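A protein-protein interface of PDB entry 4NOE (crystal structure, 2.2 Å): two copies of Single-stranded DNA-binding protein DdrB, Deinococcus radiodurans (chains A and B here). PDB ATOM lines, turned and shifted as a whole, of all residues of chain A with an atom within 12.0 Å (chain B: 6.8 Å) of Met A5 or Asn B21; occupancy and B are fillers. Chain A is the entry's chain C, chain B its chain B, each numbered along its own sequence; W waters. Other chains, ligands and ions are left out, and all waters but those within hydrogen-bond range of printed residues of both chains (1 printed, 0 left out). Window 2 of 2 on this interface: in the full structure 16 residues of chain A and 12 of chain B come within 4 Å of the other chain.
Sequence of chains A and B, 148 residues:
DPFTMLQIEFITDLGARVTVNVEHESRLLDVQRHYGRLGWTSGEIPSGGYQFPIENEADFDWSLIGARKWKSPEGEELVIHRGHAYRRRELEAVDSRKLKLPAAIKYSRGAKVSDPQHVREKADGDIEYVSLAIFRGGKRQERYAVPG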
ATOM      1  N   THR A   4      -3.369  20.291  28.819  1.00  0.00           N
ATOM      2  CA  THR A   4      -4.254  19.129  28.932  1.00  0.00           C
ATOM      3  C   THR A   4      -3.446  17.841  28.999  1.00  0.00           C
ATOM      4  O   THR A   4      -3.102  17.269  27.972  1.00  0.00           O
ATOM      5  CB  THR A   4      -5.211  19.032  27.733  1.00  0.00           C
ATOM      6  N   MET A   5      -3.145  17.388  30.211  1.00  0.00           N
ATOM      7  CA  MET A   5      -2.236  16.261  30.398  1.00  0.00           C
ATOM      8  C   MET A   5      -2.820  14.902  29.987  1.00  0.00           C
ATOM      9  O   MET A   5      -4.003  14.610  30.194  1.00  0.00           O
ATOM     10  CB  MET A   5      -1.725  16.214  31.845  1.00  0.00           C
ATOM     11  N   LEU A   6      -1.968  14.082  29.385  1.00  0.00           N
ATOM     12  CA  LEU A   6      -2.336  12.730  29.003  1.00  0.00           C
ATOM     13  C   LEU A   6      -1.379  11.771  29.665  1.00  0.00           C
ATOM     14  O   LEU A   6      -0.261  12.145  30.028  1.00  0.00           O
ATOM     15  CB  LEU A   6      -2.226  12.547  27.493  1.00  0.00           C
ATOM     16  CG  LEU A   6      -3.317  13.167  26.630  1.00  0.00           C
ATOM     17  CD1 LEU A   6      -3.188  12.694  25.198  1.00  0.00           C
ATOM     18  CD2 LEU A   6      -4.653  12.787  27.183  1.00  0.00           C
ATOM     19  N   GLN A   7      -1.815  10.526  29.807  1.00  0.00           N
ATOM     20  CA  GLN A   7      -0.927   9.462  30.210  1.00  0.00           C
ATOM     21  C   GLN A   7      -0.913   8.396  29.147  1.00  0.00           C
ATOM     22  O   GLN A   7      -1.931   8.123  28.507  1.00  0.00           O
ATOM     23  CB  GLN A   7      -1.393   8.852  31.520  1.00  0.00           C
ATOM     24  CG  GLN A   7      -1.339   9.816  32.684  1.00  0.00           C
ATOM     25  CD  GLN A   7      -1.916   9.188  33.933  1.00  0.00           C
ATOM     26  OE1 GLN A   7      -1.193   8.620  34.749  1.00  0.00           O
ATOM     27  NE2 GLN A   7      -3.233   9.266  34.075  1.00  0.00           N
ATOM     28  N   ILE A   8       0.253   7.796  28.950  1.00  0.00           N
ATOM     29  CA  ILE A   8       0.351   6.658  28.064  1.00  0.00           C
ATOM     30  C   ILE A   8       1.011   5.521  28.834  1.00  0.00           C
ATOM     31  O   ILE A   8       1.952   5.741  29.603  1.00  0.00           O
ATOM     32  CB  ILE A   8       1.076   7.029  26.736  1.00  0.00           C
ATOM     33  CG1 ILE A   8       1.264   5.797  25.841  1.00  0.00           C
ATOM     34  CG2 ILE A   8       2.404   7.718  27.007  1.00  0.00           C
ATOM     35  CD1 ILE A   8       1.882   6.123  24.464  1.00  0.00           C
ATOM     36  N   GLU A   9       0.482   4.316  28.662  1.00  0.00           N
ATOM     37  CA  GLU A   9       1.018   3.148  29.335  1.00  0.00           C
ATOM     38  C   GLU A   9       1.876   2.345  28.371  1.00  0.00           C
ATOM     39  O   GLU A   9       1.432   2.033  27.272  1.00  0.00           O
ATOM     40  CB  GLU A   9      -0.127   2.280  29.855  1.00  0.00           C
ATOM     41  N   THR A  19       3.815   3.780  33.215  1.00  0.00           N
ATOM     42  CA  THR A  19       2.989   4.875  32.736  1.00  0.00           C
ATOM     43  C   THR A  19       3.804   6.168  32.716  1.00  0.00           C
ATOM     44  O   THR A  19       4.583   6.441  33.639  1.00  0.00           O
ATOM     45  CB  THR A  19       1.726   5.031  33.592  1.00  0.00           C
ATOM     46  OG1 THR A  19       1.021   3.778  33.618  1.00  0.00           O
ATOM     47  CG2 THR A  19       0.815   6.110  33.015  1.00  0.00           C
ATOM     48  N   VAL A  20       3.636   6.941  31.645  1.00  0.00           N
ATOM     49  CA  VAL A  20       4.378   8.187  31.420  1.00  0.00           C
ATOM     50  C   VAL A  20       3.368   9.335  31.279  1.00  0.00           C
ATOM     51  O   VAL A  20       2.266   9.108  30.771  1.00  0.00           O
ATOM     52  CB  VAL A  20       5.217   8.033  30.115  1.00  0.00           C
ATOM     53  CG1 VAL A  20       5.634   9.370  29.546  1.00  0.00           C
ATOM     54  CG2 VAL A  20       6.428   7.146  30.357  1.00  0.00           C
ATOM     55  N   ASN A  21       3.703  10.543  31.742  1.00  0.00           N
ATOM     56  CA  ASN A  21       2.812  11.704  31.547  1.00  0.00           C
ATOM     57  C   ASN A  21       3.197  12.507  30.318  1.00  0.00           C
ATOM     58  O   ASN A  21       4.367  12.607  29.980  1.00  0.00           O
ATOM     59  CB  ASN A  21       2.811  12.644  32.756  1.00  0.00           C
ATOM     60  CG  ASN A  21       2.281  11.988  34.000  1.00  0.00           C
ATOM     61  OD1 ASN A  21       1.194  11.409  33.995  1.00  0.00           O
ATOM     62  ND2 ASN A  21       3.047  12.063  35.077  1.00  0.00           N
ATOM     63  N   VAL A  22       2.203  13.072  29.646  1.00  0.00           N
ATOM     64  CA  VAL A  22       2.439  13.856  28.447  1.00  0.00           C
ATOM     65  C   VAL A  22       1.759  15.200  28.649  1.00  0.00           C
ATOM     66  O   VAL A  22       0.596  15.256  29.045  1.00  0.00           O
ATOM     67  CB  VAL A  22       1.860  13.169  27.194  1.00  0.00           C
ATOM     68  CG1 VAL A  22       2.105  14.029  25.960  1.00  0.00           C
ATOM     69  CG2 VAL A  22       2.472  11.791  27.011  1.00  0.00           C
ATOM     70  N   GLU A  23       2.491  16.280  28.394  1.00  0.00           N
ATOM     71  CA  GLU A  23       1.992  17.630  28.657  1.00  0.00           C
ATOM     72  C   GLU A  23       0.726  17.978  27.866  1.00  0.00           C
ATOM     73  O   GLU A  23      -0.208  18.589  28.390  1.00  0.00           O
ATOM     74  CB  GLU A  23       3.089  18.660  28.362  1.00  0.00           C
ATOM     75  N   HIS A  24       0.703  17.578  26.602  1.00  0.00           N
ATOM     76  CA  HIS A  24      -0.378  17.957  25.708  1.00  0.00           C
ATOM     77  C   HIS A  24      -0.515  16.927  24.593  1.00  0.00           C
ATOM     78  O   HIS A  24       0.471  16.316  24.190  1.00  0.00           O
ATOM     79  CB  HIS A  24      -0.074  19.337  25.127  1.00  0.00           C
ATOM     80  CG  HIS A  24      -1.166  19.885  24.265  1.00  0.00           C
ATOM     81  ND1 HIS A  24      -1.157  19.768  22.892  1.00  0.00           N
ATOM     82  CD2 HIS A  24      -2.300  20.556  24.581  1.00  0.00           C
ATOM     83  CE1 HIS A  24      -2.239  20.340  22.398  1.00  0.00           C
ATOM     84  NE2 HIS A  24      -2.950  20.825  23.400  1.00  0.00           N
ATOM     85  N   GLU A  25      -1.731  16.744  24.088  1.00  0.00           N
ATOM     86  CA  GLU A  25      -1.999  15.718  23.083  1.00  0.00           C
ATOM     87  C   GLU A  25      -1.157  15.876  21.819  1.00  0.00           C
ATOM     88  O   GLU A  25      -0.883  14.894  21.124  1.00  0.00           O
ATOM     89  CB  GLU A  25      -3.488  15.709  22.713  1.00  0.00           C
ATOM     90  N   SER A  26      -0.744  17.104  21.517  1.00  0.00           N
ATOM     91  CA  SER A  26       0.002  17.367  20.285  1.00  0.00           C
ATOM     92  C   SER A  26       1.423  16.811  20.353  1.00  0.00           C
ATOM     93  O   SER A  26       2.140  16.792  19.353  1.00  0.00           O
ATOM     94  CB  SER A  26       0.041  18.867  20.000  1.00  0.00           C
ATOM     95  OG  SER A  26       0.634  19.561  21.088  1.00  0.00           O
ATOM     96  N   ARG A  27       1.825  16.359  21.538  1.00  0.00           N
ATOM     97  CA  ARG A  27       3.164  15.818  21.751  1.00  0.00           C
ATOM     98  C   ARG A  27       3.130  14.293  21.830  1.00  0.00           C
ATOM     99  O   ARG A  27       4.179  13.639  21.882  1.00  0.00           O
ATOM    100  CB  ARG A  27       3.757  16.396  23.036  1.00  0.00           C
ATOM    101  N   LEU A  28       1.919  13.737  21.831  1.00  0.00           N
ATOM    102  CA  LEU A  28       1.717  12.297  22.023  1.00  0.00           C
ATOM    103  C   LEU A  28       2.583  11.428  21.114  1.00  0.00           C
ATOM    104  O   LEU A  28       3.243  10.491  21.575  1.00  0.00           O
ATOM    105  CB  LEU A  28       0.236  11.936  21.837  1.00  0.00           C
ATOM    106  CG  LEU A  28      -0.128  10.450  21.927  1.00  0.00           C
ATOM    107  CD1 LEU A  28       0.239   9.865  23.280  1.00  0.00           C
ATOM    108  CD2 LEU A  28      -1.605  10.254  21.663  1.00  0.00           C
ATOM    109  N   LEU A  29       2.587  11.742  19.825  1.00  0.00           N
ATOM    110  CA  LEU A  29       3.318  10.927  18.858  1.00  0.00           C
ATOM    111  C   LEU A  29       4.828  11.061  19.054  1.00  0.00           C
ATOM    112  O   LEU A  29       5.576  10.106  18.839  1.00  0.00           O
ATOM    113  CB  LEU A  29       2.899  11.277  17.423  1.00  0.00           C
ATOM    114  CG  LEU A  29       1.765  10.424  16.843  1.00  0.00           C
ATOM    115  CD1 LEU A  29       0.719  10.087  17.886  1.00  0.00           C
ATOM    116  CD2 LEU A  29       1.110  11.112  15.667  1.00  0.00           C
ATOM    117  N   VAL A  31       6.236  11.477  21.945  1.00  0.00           N
ATOM    118  CA  VAL A  31       6.518  10.641  23.104  1.00  0.00           C
ATOM    119  C   VAL A  31       6.449   9.169  22.719  1.00  0.00           C
ATOM    120  O   VAL A  31       7.234   8.342  23.204  1.00  0.00           O
ATOM    121  CB  VAL A  31       5.563  10.972  24.261  1.00  0.00           C
ATOM    122  CG1 VAL A  31       5.615   9.911  25.336  1.00  0.00           C
ATOM    123  CG2 VAL A  31       5.927  12.335  24.848  1.00  0.00           C
ATOM    124  N   MET B   5     -13.331  15.232  38.767  1.00  0.00           N
ATOM    125  CA  MET B   5     -12.456  14.746  37.704  1.00  0.00           C
ATOM    126  C   MET B   5     -12.650  13.252  37.420  1.00  0.00           C
ATOM    127  O   MET B   5     -12.580  12.420  38.329  1.00  0.00           O
ATOM    128  CB  MET B   5     -10.990  15.020  38.051  1.00  0.00           C
ATOM    129  N   LEU B   6     -12.908  12.933  36.155  1.00  0.00           N
ATOM    130  CA  LEU B   6     -12.900  11.559  35.669  1.00  0.00           C
ATOM    131  C   LEU B   6     -11.675  11.339  34.785  1.00  0.00           C
ATOM    132  O   LEU B   6     -11.046  12.289  34.314  1.00  0.00           O
ATOM    133  CB  LEU B   6     -14.145  11.268  34.833  1.00  0.00           C
ATOM    134  CG  LEU B   6     -15.539  11.390  35.433  1.00  0.00           C
ATOM    135  CD1 LEU B   6     -16.509  11.632  34.310  1.00  0.00           C
ATOM    136  CD2 LEU B   6     -15.906  10.128  36.147  1.00  0.00           C
ATOM    137  N   GLN B   7     -11.357  10.074  34.555  1.00  0.00           N
ATOM    138  CA  GLN B   7     -10.312   9.688  33.626  1.00  0.00           C
ATOM    139  C   GLN B   7     -10.920   8.667  32.695  1.00  0.00           C
ATOM    140  O   GLN B   7     -11.670   7.793  33.131  1.00  0.00           O
ATOM    141  CB  GLN B   7      -9.132   9.058  34.371  1.00  0.00           C
ATOM    142  CG  GLN B   7      -8.260  10.072  35.111  1.00  0.00           C
ATOM    143  CD  GLN B   7      -7.135   9.411  35.882  1.00  0.00           C
ATOM    144  OE1 GLN B   7      -6.003   9.331  35.405  1.00  0.00           O
ATOM    145  NE2 GLN B   7      -7.441   8.933  37.082  1.00  0.00           N
ATOM    146  N   ILE B   8     -10.620   8.790  31.410  1.00  0.00           N
ATOM    147  CA  ILE B   8     -11.072   7.797  30.460  1.00  0.00           C
ATOM    148  C   ILE B   8      -9.883   7.258  29.689  1.00  0.00           C
ATOM    149  O   ILE B   8      -9.039   8.022  29.190  1.00  0.00           O
ATOM    150  CB  ILE B   8     -12.172   8.350  29.518  1.00  0.00           C
ATOM    151  CG1 ILE B   8     -12.475   7.338  28.413  1.00  0.00           C
ATOM    152  CG2 ILE B   8     -11.779   9.705  28.935  1.00  0.00           C
ATOM    153  CD1 ILE B   8     -13.773   7.635  27.655  1.00  0.00           C
ATOM    154  N   THR B  19      -4.635   7.662  28.549  1.00  0.00           N
ATOM    155  CA  THR B  19      -5.659   8.066  29.505  1.00  0.00           C
ATOM    156  C   THR B  19      -5.842   9.567  29.414  1.00  0.00           C
ATOM    157  O   THR B  19      -4.861  10.328  29.479  1.00  0.00           O
ATOM    158  CB  THR B  19      -5.263   7.692  30.953  1.00  0.00           C
ATOM    159  OG1 THR B  19      -5.075   6.274  31.049  1.00  0.00           O
ATOM    160  CG2 THR B  19      -6.340   8.104  31.930  1.00  0.00           C
ATOM    161  N   VAL B  20      -7.098   9.987  29.283  1.00  0.00           N
ATOM    162  CA  VAL B  20      -7.471  11.391  29.177  1.00  0.00           C
ATOM    163  C   VAL B  20      -8.193  11.842  30.449  1.00  0.00           C
ATOM    164  O   VAL B  20      -9.081  11.145  30.938  1.00  0.00           O
ATOM    165  CB  VAL B  20      -8.422  11.590  27.970  1.00  0.00           C
ATOM    166  CG1 VAL B  20      -8.987  13.000  27.933  1.00  0.00           C
ATOM    167  CG2 VAL B  20      -7.703  11.259  26.665  1.00  0.00           C
ATOM    168  N   ASN B  21      -7.810  13.004  30.977  1.00  0.00           N
ATOM    169  CA  ASN B  21      -8.487  13.614  32.121  1.00  0.00           C
ATOM    170  C   ASN B  21      -9.666  14.483  31.697  1.00  0.00           C
ATOM    171  O   ASN B  21      -9.560  15.287  30.764  1.00  0.00           O
ATOM    172  CB  ASN B  21      -7.510  14.461  32.934  1.00  0.00           C
ATOM    173  CG  ASN B  21      -6.338  13.657  33.443  1.00  0.00           C
ATOM    174  OD1 ASN B  21      -6.445  12.956  34.446  1.00  0.00           O
ATOM    175  ND2 ASN B  21      -5.212  13.744  32.744  1.00  0.00           N
ATOM    176  N   VAL B  22     -10.789  14.312  32.388  1.00  0.00           N
ATOM    177  CA  VAL B  22     -12.023  15.012  32.050  1.00  0.00           C
ATOM    178  C   VAL B  22     -12.476  15.821  33.252  1.00  0.00           C
ATOM    179  O   VAL B  22     -12.800  15.261  34.307  1.00  0.00           O
ATOM    180  CB  VAL B  22     -13.136  14.030  31.687  1.00  0.00           C
ATOM    181  CG1 VAL B  22     -14.445  14.778  31.483  1.00  0.00           C
ATOM    182  CG2 VAL B  22     -12.761  13.244  30.438  1.00  0.00           C
ATOM    183  N   GLU B  23     -12.502  17.138  33.094  1.00  0.00           N
ATOM    184  CA  GLU B  23     -12.778  18.027  34.215  1.00  0.00           C
ATOM    185  C   GLU B  23     -14.183  17.831  34.768  1.00  0.00           C
ATOM    186  O   GLU B  23     -14.371  17.764  35.984  1.00  0.00           O
ATOM    187  CB  GLU B  23     -12.549  19.486  33.812  1.00  0.00           C
ATOM    188  N   HIS B  24     -15.160  17.708  33.873  1.00  0.00           N
ATOM    189  CA  HIS B  24     -16.563  17.634  34.278  1.00  0.00           C
ATOM    190  C   HIS B  24     -17.318  16.461  33.645  1.00  0.00           C
ATOM    191  O   HIS B  24     -17.315  16.292  32.412  1.00  0.00           O
ATOM    192  CB  HIS B  24     -17.280  18.947  33.938  1.00  0.00           C
ATOM    193  CG  HIS B  24     -16.727  20.143  34.651  1.00  0.00           C
ATOM    194  ND1 HIS B  24     -15.983  21.114  34.010  1.00  0.00           N
ATOM    195  CD2 HIS B  24     -16.806  20.525  35.949  1.00  0.00           C
ATOM    196  CE1 HIS B  24     -15.630  22.041  34.881  1.00  0.00           C
ATOM    197  NE2 HIS B  24     -16.113  21.709  36.067  1.00  0.00           N
ATOM    198  N   VAL B  31     -16.164  14.317  25.155  1.00  0.00           N
ATOM    199  CA  VAL B  31     -14.797  13.831  25.065  1.00  0.00           C
ATOM    200  C   VAL B  31     -14.698  12.522  24.259  1.00  0.00           C
ATOM    201  O   VAL B  31     -13.768  12.346  23.464  1.00  0.00           O
ATOM    202  CB  VAL B  31     -14.183  13.696  26.476  1.00  0.00           C
ATOM    203  CG1 VAL B  31     -12.850  12.991  26.425  1.00  0.00           C
ATOM    204  CG2 VAL B  31     -14.023  15.092  27.092  1.00  0.00           C
HETATM  205  O   HOH W   1      -6.225  15.078  29.259  1.00  0.00           O
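Water W1 lies within hydrogen-bond range of the backbone carbonyl oxygen of Met A5 (2.5 Å) and the backbone NH of Asn B21 (3.1 Å).
Among the printed residues, pairs that only touch across the chains: Leu A6 with Thr B19 and Leu A6 with Val B20.
The backbone carbonyl oxygen (O) of Ile B8 lies within hydrogen-bond range of the backbone NH (N) of Val B20.
The backbone NH (N) of Val A22 lies within hydrogen-bond range of the backbone carbonyl oxygen (O) of Leu A6, 2.7 Å away.
Met A5 touches just one residue of chain B: Asn B21.
Printed residues of chain B within 4 Å of Leu A6: Thr B19 (3.4 Å) and Val B20 (3.5 Å).
Printed residues of chain B within 4 Å of Gln A7: Gln B7 and Thr B19.
Gln B7 touches just one residue of chain A: Gln A7 (3.1 Å).
Of chain A, only Leu A6 (3.5 Å) comes within 4 Å of Val B20.
Of chain A, only Met A5 (3.0 Å) comes within 4 Å of Asn B21.
No residue of chain A comes within 4 Å of Glu B23.
The nearest residue of chain B that does not touch Met A5 is Thr B19 (4.4 Å).
Met A5 touches Asn B21, but with the chains exchanged Asn A21 does not touch Met B5 (13.3 Å).
Leu A6 touches Thr B19, but with the chains exchanged Thr A19 does not touch Leu B6 (13.4 Å).
Leu A6 touches Val B20, but with the chains exchanged Val A20 does not touch Leu B6 (14.1 Å).
Gln B7 touches its own counterpart, Gln A7.
11 positions are printed for both chains.
Of the 5 pairs that touch across the chains among the printed residues, 1 has its exchanged pair printed and touching as well.
Of the 11 printed residues of chain B, 4 touch a printed residue of chain A.
Printed residues of chain B that touch a printed residue of chain A: Gln B7, Thr B19, Val B20 and Asn B21.
Hydrophobic or aromatic side chains of chain A that line the printed part of chain B: Leu A6.
Along chain A the printed residues that touch a printed residue of chain B span positions 5 to 7.
The side-chain amide oxygen (OE1) of Gln B7 sits at hydrogen-bond distance from the side-chain amide nitrogen (NE2) of Gln A7 (3.1 Å).
The backbone NH (N) of Thr B19 sits at hydrogen-bond distance from the backbone carbonyl oxygen (O) of Gln A7, 2.7 Å away.
The backbone carbonyl oxygen (O) of Met A5 sits at hydrogen-bond distance from the side-chain amide nitrogen (ND2) of Asn B21, 3.0 Å away.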
